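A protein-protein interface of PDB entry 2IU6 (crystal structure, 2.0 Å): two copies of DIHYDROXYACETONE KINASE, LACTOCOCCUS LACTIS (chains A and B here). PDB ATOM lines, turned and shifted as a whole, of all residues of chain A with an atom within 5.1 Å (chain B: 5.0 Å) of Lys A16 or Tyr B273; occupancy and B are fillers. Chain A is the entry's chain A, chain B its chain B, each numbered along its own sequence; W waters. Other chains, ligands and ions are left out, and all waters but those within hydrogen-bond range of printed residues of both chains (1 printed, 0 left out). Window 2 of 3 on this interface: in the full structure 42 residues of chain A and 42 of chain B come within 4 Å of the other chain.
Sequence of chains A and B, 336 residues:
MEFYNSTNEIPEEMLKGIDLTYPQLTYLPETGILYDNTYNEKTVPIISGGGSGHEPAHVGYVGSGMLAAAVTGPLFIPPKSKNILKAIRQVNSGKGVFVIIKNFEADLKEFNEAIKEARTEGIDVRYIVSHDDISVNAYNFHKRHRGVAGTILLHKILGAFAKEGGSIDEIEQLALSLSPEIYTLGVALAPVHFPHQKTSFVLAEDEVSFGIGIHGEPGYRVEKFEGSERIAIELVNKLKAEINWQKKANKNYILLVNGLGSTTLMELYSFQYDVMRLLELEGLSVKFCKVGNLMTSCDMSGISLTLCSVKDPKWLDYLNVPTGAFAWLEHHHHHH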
ATOM      1  N   GLU A  12      -3.373  14.962  -3.968  1.00  0.00           N
ATOM      2  CA  GLU A  12      -3.574  16.007  -4.949  1.00  0.00           C
ATOM      3  C   GLU A  12      -2.910  17.312  -4.479  1.00  0.00           C
ATOM      4  O   GLU A  12      -2.244  17.996  -5.256  1.00  0.00           O
ATOM      5  CB  GLU A  12      -5.073  16.156  -5.206  1.00  0.00           C
ATOM      6  CG  GLU A  12      -5.401  17.117  -6.323  1.00  0.00           C
ATOM      7  CD  GLU A  12      -5.303  16.474  -7.698  1.00  0.00           C
ATOM      8  OE1 GLU A  12      -4.845  15.306  -7.821  1.00  0.00           O
ATOM      9  OE2 GLU A  12      -5.696  17.159  -8.662  1.00  0.00           O
ATOM     10  N   GLU A  13      -3.071  17.670  -3.213  1.00  0.00           N
ATOM     11  CA  GLU A  13      -2.473  18.918  -2.729  1.00  0.00           C
ATOM     12  C   GLU A  13      -0.945  18.843  -2.755  1.00  0.00           C
ATOM     13  O   GLU A  13      -0.259  19.813  -3.086  1.00  0.00           O
ATOM     14  CB  GLU A  13      -2.934  19.213  -1.302  1.00  0.00           C
ATOM     15  CG  GLU A  13      -4.426  19.417  -1.168  1.00  0.00           C
ATOM     16  CD  GLU A  13      -5.221  18.148  -1.442  1.00  0.00           C
ATOM     17  OE1 GLU A  13      -4.843  17.056  -0.960  1.00  0.00           O
ATOM     18  OE2 GLU A  13      -6.235  18.259  -2.151  1.00  0.00           O
ATOM     19  N   MET A  14      -0.410  17.681  -2.400  1.00  0.00           N
ATOM     20  CA  MET A  14       1.034  17.495  -2.437  1.00  0.00           C
ATOM     21  C   MET A  14       1.558  17.764  -3.853  1.00  0.00           C
ATOM     22  O   MET A  14       2.545  18.493  -4.059  1.00  0.00           O
ATOM     23  CB  MET A  14       1.403  16.066  -2.030  1.00  0.00           C
ATOM     24  CG  MET A  14       2.894  15.772  -2.187  1.00  0.00           C
ATOM     25  SD  MET A  14       3.326  14.038  -2.088  1.00  0.00           S
ATOM     26  CE  MET A  14       3.077  13.499  -3.796  1.00  0.00           C
ATOM     27  N   LEU A  15       0.888  17.163  -4.826  1.00  0.00           N
ATOM     28  CA  LEU A  15       1.289  17.290  -6.227  1.00  0.00           C
ATOM     29  C   LEU A  15       1.168  18.729  -6.720  1.00  0.00           C
ATOM     30  O   LEU A  15       2.045  19.219  -7.434  1.00  0.00           O
ATOM     31  CB  LEU A  15       0.489  16.315  -7.097  1.00  0.00           C
ATOM     32  CG  LEU A  15       0.797  14.847  -6.724  1.00  0.00           C
ATOM     33  CD1 LEU A  15      -0.278  13.854  -7.125  1.00  0.00           C
ATOM     34  CD2 LEU A  15       2.135  14.411  -7.320  1.00  0.00           C
ATOM     35  N   LYS A  16       0.090  19.411  -6.341  1.00  0.00           N
ATOM     36  CA  LYS A  16      -0.069  20.818  -6.651  1.00  0.00           C
ATOM     37  C   LYS A  16       1.004  21.679  -6.011  1.00  0.00           C
ATOM     38  O   LYS A  16       1.533  22.614  -6.634  1.00  0.00           O
ATOM     39  CB  LYS A  16      -1.461  21.289  -6.238  1.00  0.00           C
ATOM     40  CG  LYS A  16      -2.543  20.649  -7.123  1.00  0.00           C
ATOM     41  CD  LYS A  16      -3.799  21.469  -7.156  1.00  0.00           C
ATOM     42  CE  LYS A  16      -4.793  21.026  -6.105  1.00  0.00           C
ATOM     43  NZ  LYS A  16      -6.180  20.963  -6.708  1.00  0.00           N
ATOM     44  N   GLY A  17       1.325  21.362  -4.764  1.00  0.00           N
ATOM     45  CA  GLY A  17       2.413  22.025  -4.053  1.00  0.00           C
ATOM     46  C   GLY A  17       3.757  21.858  -4.735  1.00  0.00           C
ATOM     47  O   GLY A  17       4.524  22.814  -4.849  1.00  0.00           O
ATOM     48  N   ILE A  18       4.059  20.649  -5.188  1.00  0.00           N
ATOM     49  CA  ILE A  18       5.321  20.392  -5.875  1.00  0.00           C
ATOM     50  C   ILE A  18       5.356  21.248  -7.151  1.00  0.00           C
ATOM     51  O   ILE A  18       6.361  21.889  -7.481  1.00  0.00           O
ATOM     52  CB  ILE A  18       5.452  18.901  -6.187  1.00  0.00           C
ATOM     53  CG1 ILE A  18       5.737  18.135  -4.895  1.00  0.00           C
ATOM     54  CG2 ILE A  18       6.568  18.641  -7.190  1.00  0.00           C
ATOM     55  CD1 ILE A  18       5.620  16.623  -5.087  1.00  0.00           C
ATOM     56  N   ASP A  19       4.238  21.261  -7.863  1.00  0.00           N
ATOM     57  CA  ASP A  19       4.098  22.124  -9.041  1.00  0.00           C
ATOM     58  C   ASP A  19       4.384  23.624  -8.798  1.00  0.00           C
ATOM     59  O   ASP A  19       5.205  24.230  -9.502  1.00  0.00           O
ATOM     60  CB  ASP A  19       2.765  21.845  -9.749  1.00  0.00           C
ATOM     61  CG  ASP A  19       2.629  22.596 -11.069  1.00  0.00           C
ATOM     62  OD1 ASP A  19       3.566  23.364 -11.409  1.00  0.00           O
ATOM     63  OD2 ASP A  19       1.581  22.407 -11.742  1.00  0.00           O
ATOM     64  N   LEU A  20       3.724  24.230  -7.809  1.00  0.00           N
ATOM     65  CA  LEU A  20       4.046  25.596  -7.379  1.00  0.00           C
ATOM     66  C   LEU A  20       5.509  25.843  -6.999  1.00  0.00           C
ATOM     67  O   LEU A  20       6.051  26.916  -7.259  1.00  0.00           O
ATOM     68  CB  LEU A  20       3.213  25.979  -6.163  1.00  0.00           C
ATOM     69  CG  LEU A  20       1.743  26.106  -6.524  1.00  0.00           C
ATOM     70  CD1 LEU A  20       0.968  26.146  -5.214  1.00  0.00           C
ATOM     71  CD2 LEU A  20       1.520  27.381  -7.328  1.00  0.00           C
ATOM     72  N   TYR A  27       2.093  19.565 -12.874  1.00  0.00           N
ATOM     73  CA  TYR A  27       1.187  18.517 -12.432  1.00  0.00           C
ATOM     74  C   TYR A  27      -0.155  18.583 -13.171  1.00  0.00           C
ATOM     75  O   TYR A  27      -0.684  19.657 -13.425  1.00  0.00           O
ATOM     76  CB  TYR A  27       0.950  18.575 -10.915  1.00  0.00           C
ATOM     77  CG  TYR A  27      -0.097  17.582 -10.508  1.00  0.00           C
ATOM     78  CD1 TYR A  27       0.089  16.224 -10.767  1.00  0.00           C
ATOM     79  CD2 TYR A  27      -1.279  17.989  -9.881  1.00  0.00           C
ATOM     80  CE1 TYR A  27      -0.861  15.295 -10.418  1.00  0.00           C
ATOM     81  CE2 TYR A  27      -2.246  17.057  -9.521  1.00  0.00           C
ATOM     82  CZ  TYR A  27      -2.023  15.716  -9.799  1.00  0.00           C
ATOM     83  OH  TYR A  27      -2.953  14.778  -9.456  1.00  0.00           O
ATOM     84  N   TYR B 269       4.629  19.321   1.309  1.00  0.00           N
ATOM     85  CA  TYR B 269       4.111  19.914   0.069  1.00  0.00           C
ATOM     86  C   TYR B 269       2.595  20.131   0.104  1.00  0.00           C
ATOM     87  O   TYR B 269       2.092  21.107  -0.452  1.00  0.00           O
ATOM     88  CB  TYR B 269       4.542  19.086  -1.157  1.00  0.00           C
ATOM     89  CG  TYR B 269       6.004  19.274  -1.505  1.00  0.00           C
ATOM     90  CD1 TYR B 269       6.952  18.332  -1.133  1.00  0.00           C
ATOM     91  CD2 TYR B 269       6.443  20.392  -2.212  1.00  0.00           C
ATOM     92  CE1 TYR B 269       8.332  18.500  -1.459  1.00  0.00           C
ATOM     93  CE2 TYR B 269       7.802  20.575  -2.537  1.00  0.00           C
ATOM     94  CZ  TYR B 269       8.748  19.619  -2.158  1.00  0.00           C
ATOM     95  OH  TYR B 269      10.110  19.761  -2.456  1.00  0.00           O
ATOM     96  N   SER B 270       1.835  19.252   0.749  1.00  0.00           N
ATOM     97  CA  SER B 270       0.410  19.530   0.976  1.00  0.00           C
ATOM     98  C   SER B 270       0.205  20.828   1.780  1.00  0.00           C
ATOM     99  O   SER B 270      -0.705  21.643   1.499  1.00  0.00           O
ATOM    100  CB  SER B 270      -0.279  18.399   1.735  1.00  0.00           C
ATOM    101  OG  SER B 270      -0.160  17.188   1.044  1.00  0.00           O
ATOM    102  N   PHE B 271       1.042  21.016   2.795  1.00  0.00           N
ATOM    103  CA  PHE B 271       0.962  22.225   3.613  1.00  0.00           C
ATOM    104  C   PHE B 271       1.377  23.471   2.829  1.00  0.00           C
ATOM    105  O   PHE B 271       0.689  24.494   2.876  1.00  0.00           O
ATOM    106  CB  PHE B 271       1.882  22.124   4.846  1.00  0.00           C
ATOM    107  CG  PHE B 271       1.476  23.063   5.956  1.00  0.00           C
ATOM    108  CD1 PHE B 271       0.248  22.910   6.588  1.00  0.00           C
ATOM    109  CD2 PHE B 271       2.303  24.080   6.351  1.00  0.00           C
ATOM    110  CE1 PHE B 271      -0.130  23.773   7.611  1.00  0.00           C
ATOM    111  CE2 PHE B 271       1.939  24.960   7.382  1.00  0.00           C
ATOM    112  CZ  PHE B 271       0.725  24.809   8.011  1.00  0.00           C
ATOM    113  N   GLN B 272       2.496  23.381   2.118  1.00  0.00           N
ATOM    114  CA  GLN B 272       2.869  24.414   1.141  1.00  0.00           C
ATOM    115  C   GLN B 272       1.720  24.827   0.204  1.00  0.00           C
ATOM    116  O   GLN B 272       1.493  26.012  -0.065  1.00  0.00           O
ATOM    117  CB  GLN B 272       4.109  23.948   0.365  1.00  0.00           C
ATOM    118  CG  GLN B 272       4.180  24.374  -1.084  1.00  0.00           C
ATOM    119  CD  GLN B 272       4.918  25.665  -1.208  1.00  0.00           C
ATOM    120  OE1 GLN B 272       4.986  26.420  -0.245  1.00  0.00           O
ATOM    121  NE2 GLN B 272       5.474  25.942  -2.385  1.00  0.00           N
ATOM    122  N   TYR B 273       0.979  23.856  -0.309  1.00  0.00           N
ATOM    123  CA  TYR B 273      -0.145  24.177  -1.151  1.00  0.00           C
ATOM    124  C   TYR B 273      -1.181  25.034  -0.398  1.00  0.00           C
ATOM    125  O   TYR B 273      -1.627  26.056  -0.924  1.00  0.00           O
ATOM    126  CB  TYR B 273      -0.775  22.920  -1.753  1.00  0.00           C
ATOM    127  CG  TYR B 273      -2.115  23.206  -2.404  1.00  0.00           C
ATOM    128  CD1 TYR B 273      -2.193  23.788  -3.674  1.00  0.00           C
ATOM    129  CD2 TYR B 273      -3.297  22.902  -1.756  1.00  0.00           C
ATOM    130  CE1 TYR B 273      -3.426  24.054  -4.267  1.00  0.00           C
ATOM    131  CE2 TYR B 273      -4.537  23.166  -2.343  1.00  0.00           C
ATOM    132  CZ  TYR B 273      -4.592  23.737  -3.594  1.00  0.00           C
ATOM    133  OH  TYR B 273      -5.838  23.991  -4.162  1.00  0.00           O
ATOM    134  N   ASP B 274      -1.564  24.636   0.818  1.00  0.00           N
ATOM    135  CA  ASP B 274      -2.550  25.400   1.585  1.00  0.00           C
ATOM    136  C   ASP B 274      -2.024  26.800   1.894  1.00  0.00           C
ATOM    137  O   ASP B 274      -2.764  27.786   1.775  1.00  0.00           O
ATOM    138  CB  ASP B 274      -2.948  24.674   2.889  1.00  0.00           C
ATOM    139  CG  ASP B 274      -3.910  23.522   2.656  1.00  0.00           C
ATOM    140  OD1 ASP B 274      -4.716  23.611   1.708  1.00  0.00           O
ATOM    141  OD2 ASP B 274      -3.873  22.513   3.411  1.00  0.00           O
ATOM    142  N   VAL B 275      -0.755  26.898   2.286  1.00  0.00           N
ATOM    143  CA  VAL B 275      -0.135  28.189   2.617  1.00  0.00           C
ATOM    144  C   VAL B 275      -0.026  29.153   1.411  1.00  0.00           C
ATOM    145  O   VAL B 275      -0.387  30.340   1.484  1.00  0.00           O
ATOM    146  CB  VAL B 275       1.265  27.986   3.243  1.00  0.00           C
ATOM    147  CG1 VAL B 275       2.009  29.328   3.430  1.00  0.00           C
ATOM    148  CG2 VAL B 275       1.140  27.243   4.588  1.00  0.00           C
ATOM    149  N   MET B 276       0.474  28.650   0.292  1.00  0.00           N
ATOM    150  CA  MET B 276       0.472  29.416  -0.944  1.00  0.00           C
ATOM    151  C   MET B 276      -0.900  29.937  -1.363  1.00  0.00           C
ATOM    152  O   MET B 276      -0.990  31.079  -1.819  1.00  0.00           O
ATOM    153  CB  MET B 276       1.054  28.598  -2.098  1.00  0.00           C
ATOM    154  CG  MET B 276       2.533  28.162  -1.945  1.00  0.00           C
ATOM    155  SD  MET B 276       3.734  29.450  -2.320  1.00  0.00           S
ATOM    156  CE  MET B 276       3.652  29.661  -4.094  1.00  0.00           C
ATOM    157  N   ARG B 277      -1.961  29.134  -1.227  1.00  0.00           N
ATOM    158  CA  ARG B 277      -3.310  29.606  -1.556  1.00  0.00           C
ATOM    159  C   ARG B 277      -3.742  30.752  -0.633  1.00  0.00           C
ATOM    160  O   ARG B 277      -4.338  31.747  -1.080  1.00  0.00           O
ATOM    161  CB  ARG B 277      -4.346  28.475  -1.506  1.00  0.00           C
ATOM    162  CG  ARG B 277      -4.270  27.435  -2.638  1.00  0.00           C
ATOM    163  CD  ARG B 277      -5.027  27.848  -3.900  1.00  0.00           C
ATOM    164  NE  ARG B 277      -6.278  27.108  -4.118  1.00  0.00           N
ATOM    165  CZ  ARG B 277      -7.357  27.599  -4.733  1.00  0.00           C
ATOM    166  NH1 ARG B 277      -7.362  28.844  -5.203  1.00  0.00           N
ATOM    167  NH2 ARG B 277      -8.447  26.849  -4.884  1.00  0.00           N
HETATM  168  O   HOH W   1      -1.957  15.665  -0.656  1.00  0.00           O
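Water W1 lies within hydrogen-bond range of OG of Ser B270 (2.9 Å), N of Met A14 (3.1 Å) and OE1 of Glu A13 (3.2 Å).
Of the 10 printed residues of chain A, 6 touch a printed residue of chain B.
Hydrophobic or aromatic side chains of chain B that line the printed part of chain A: Tyr B269, Tyr B273 and Met B276.
Among the printed residues, 9 pairs touch across the chains.
Among the printed residues, no Asp or Glu carboxylate lies within 4 Å of a Lys or Arg side-chain nitrogen of the other chain.
Among the printed residues, merely in contact across the chains: Glu A13 with Tyr B269 (3.8 Å), Glu A13 with Tyr B273 (3.4 Å), Met A14 with Tyr B269 (3.6 Å), Lys A16 with Tyr B273 (3.7 Å), Gly A17 with Tyr B269 (3.7 Å), Gly A17 with Tyr B273 (3.99 Å), Ile A18 with Tyr B269 (3.6 Å) and Leu A20 with Met B276 (3.97 Å).
The side-chain hydroxyl of Ser B270 is in hydrogen-bond range of the backbone NH of Met A14 (3.5 Å).
Of the printed residues of chain B, Glu A13 touches Tyr B269 and Tyr B273.
Of chain B, only Tyr B273 comes within 4 Å of Lys A16.
Printed residues of chain B within 4 Å of Leu A20: Met B276 (3.97 Å).
Of the printed residues of chain A, Ser B270 touches Met A14 (3.5 Å).
Printed residues of chain A within 4 Å of Tyr B273: Glu A13, Lys A16 and Gly A17.
The nearest printed residue of chain B that does not touch Gly A17 is Gln B272 (4.1 Å).
The side-chain hydroxyl (OH) of Tyr B273 lies within hydrogen-bond range of the guanidinium group (NE) of Arg B277.
No position is printed for both chains.
Of the 9 pairs that touch across the chains among the printed residues, none has its exchanged pair printed and touching as well.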
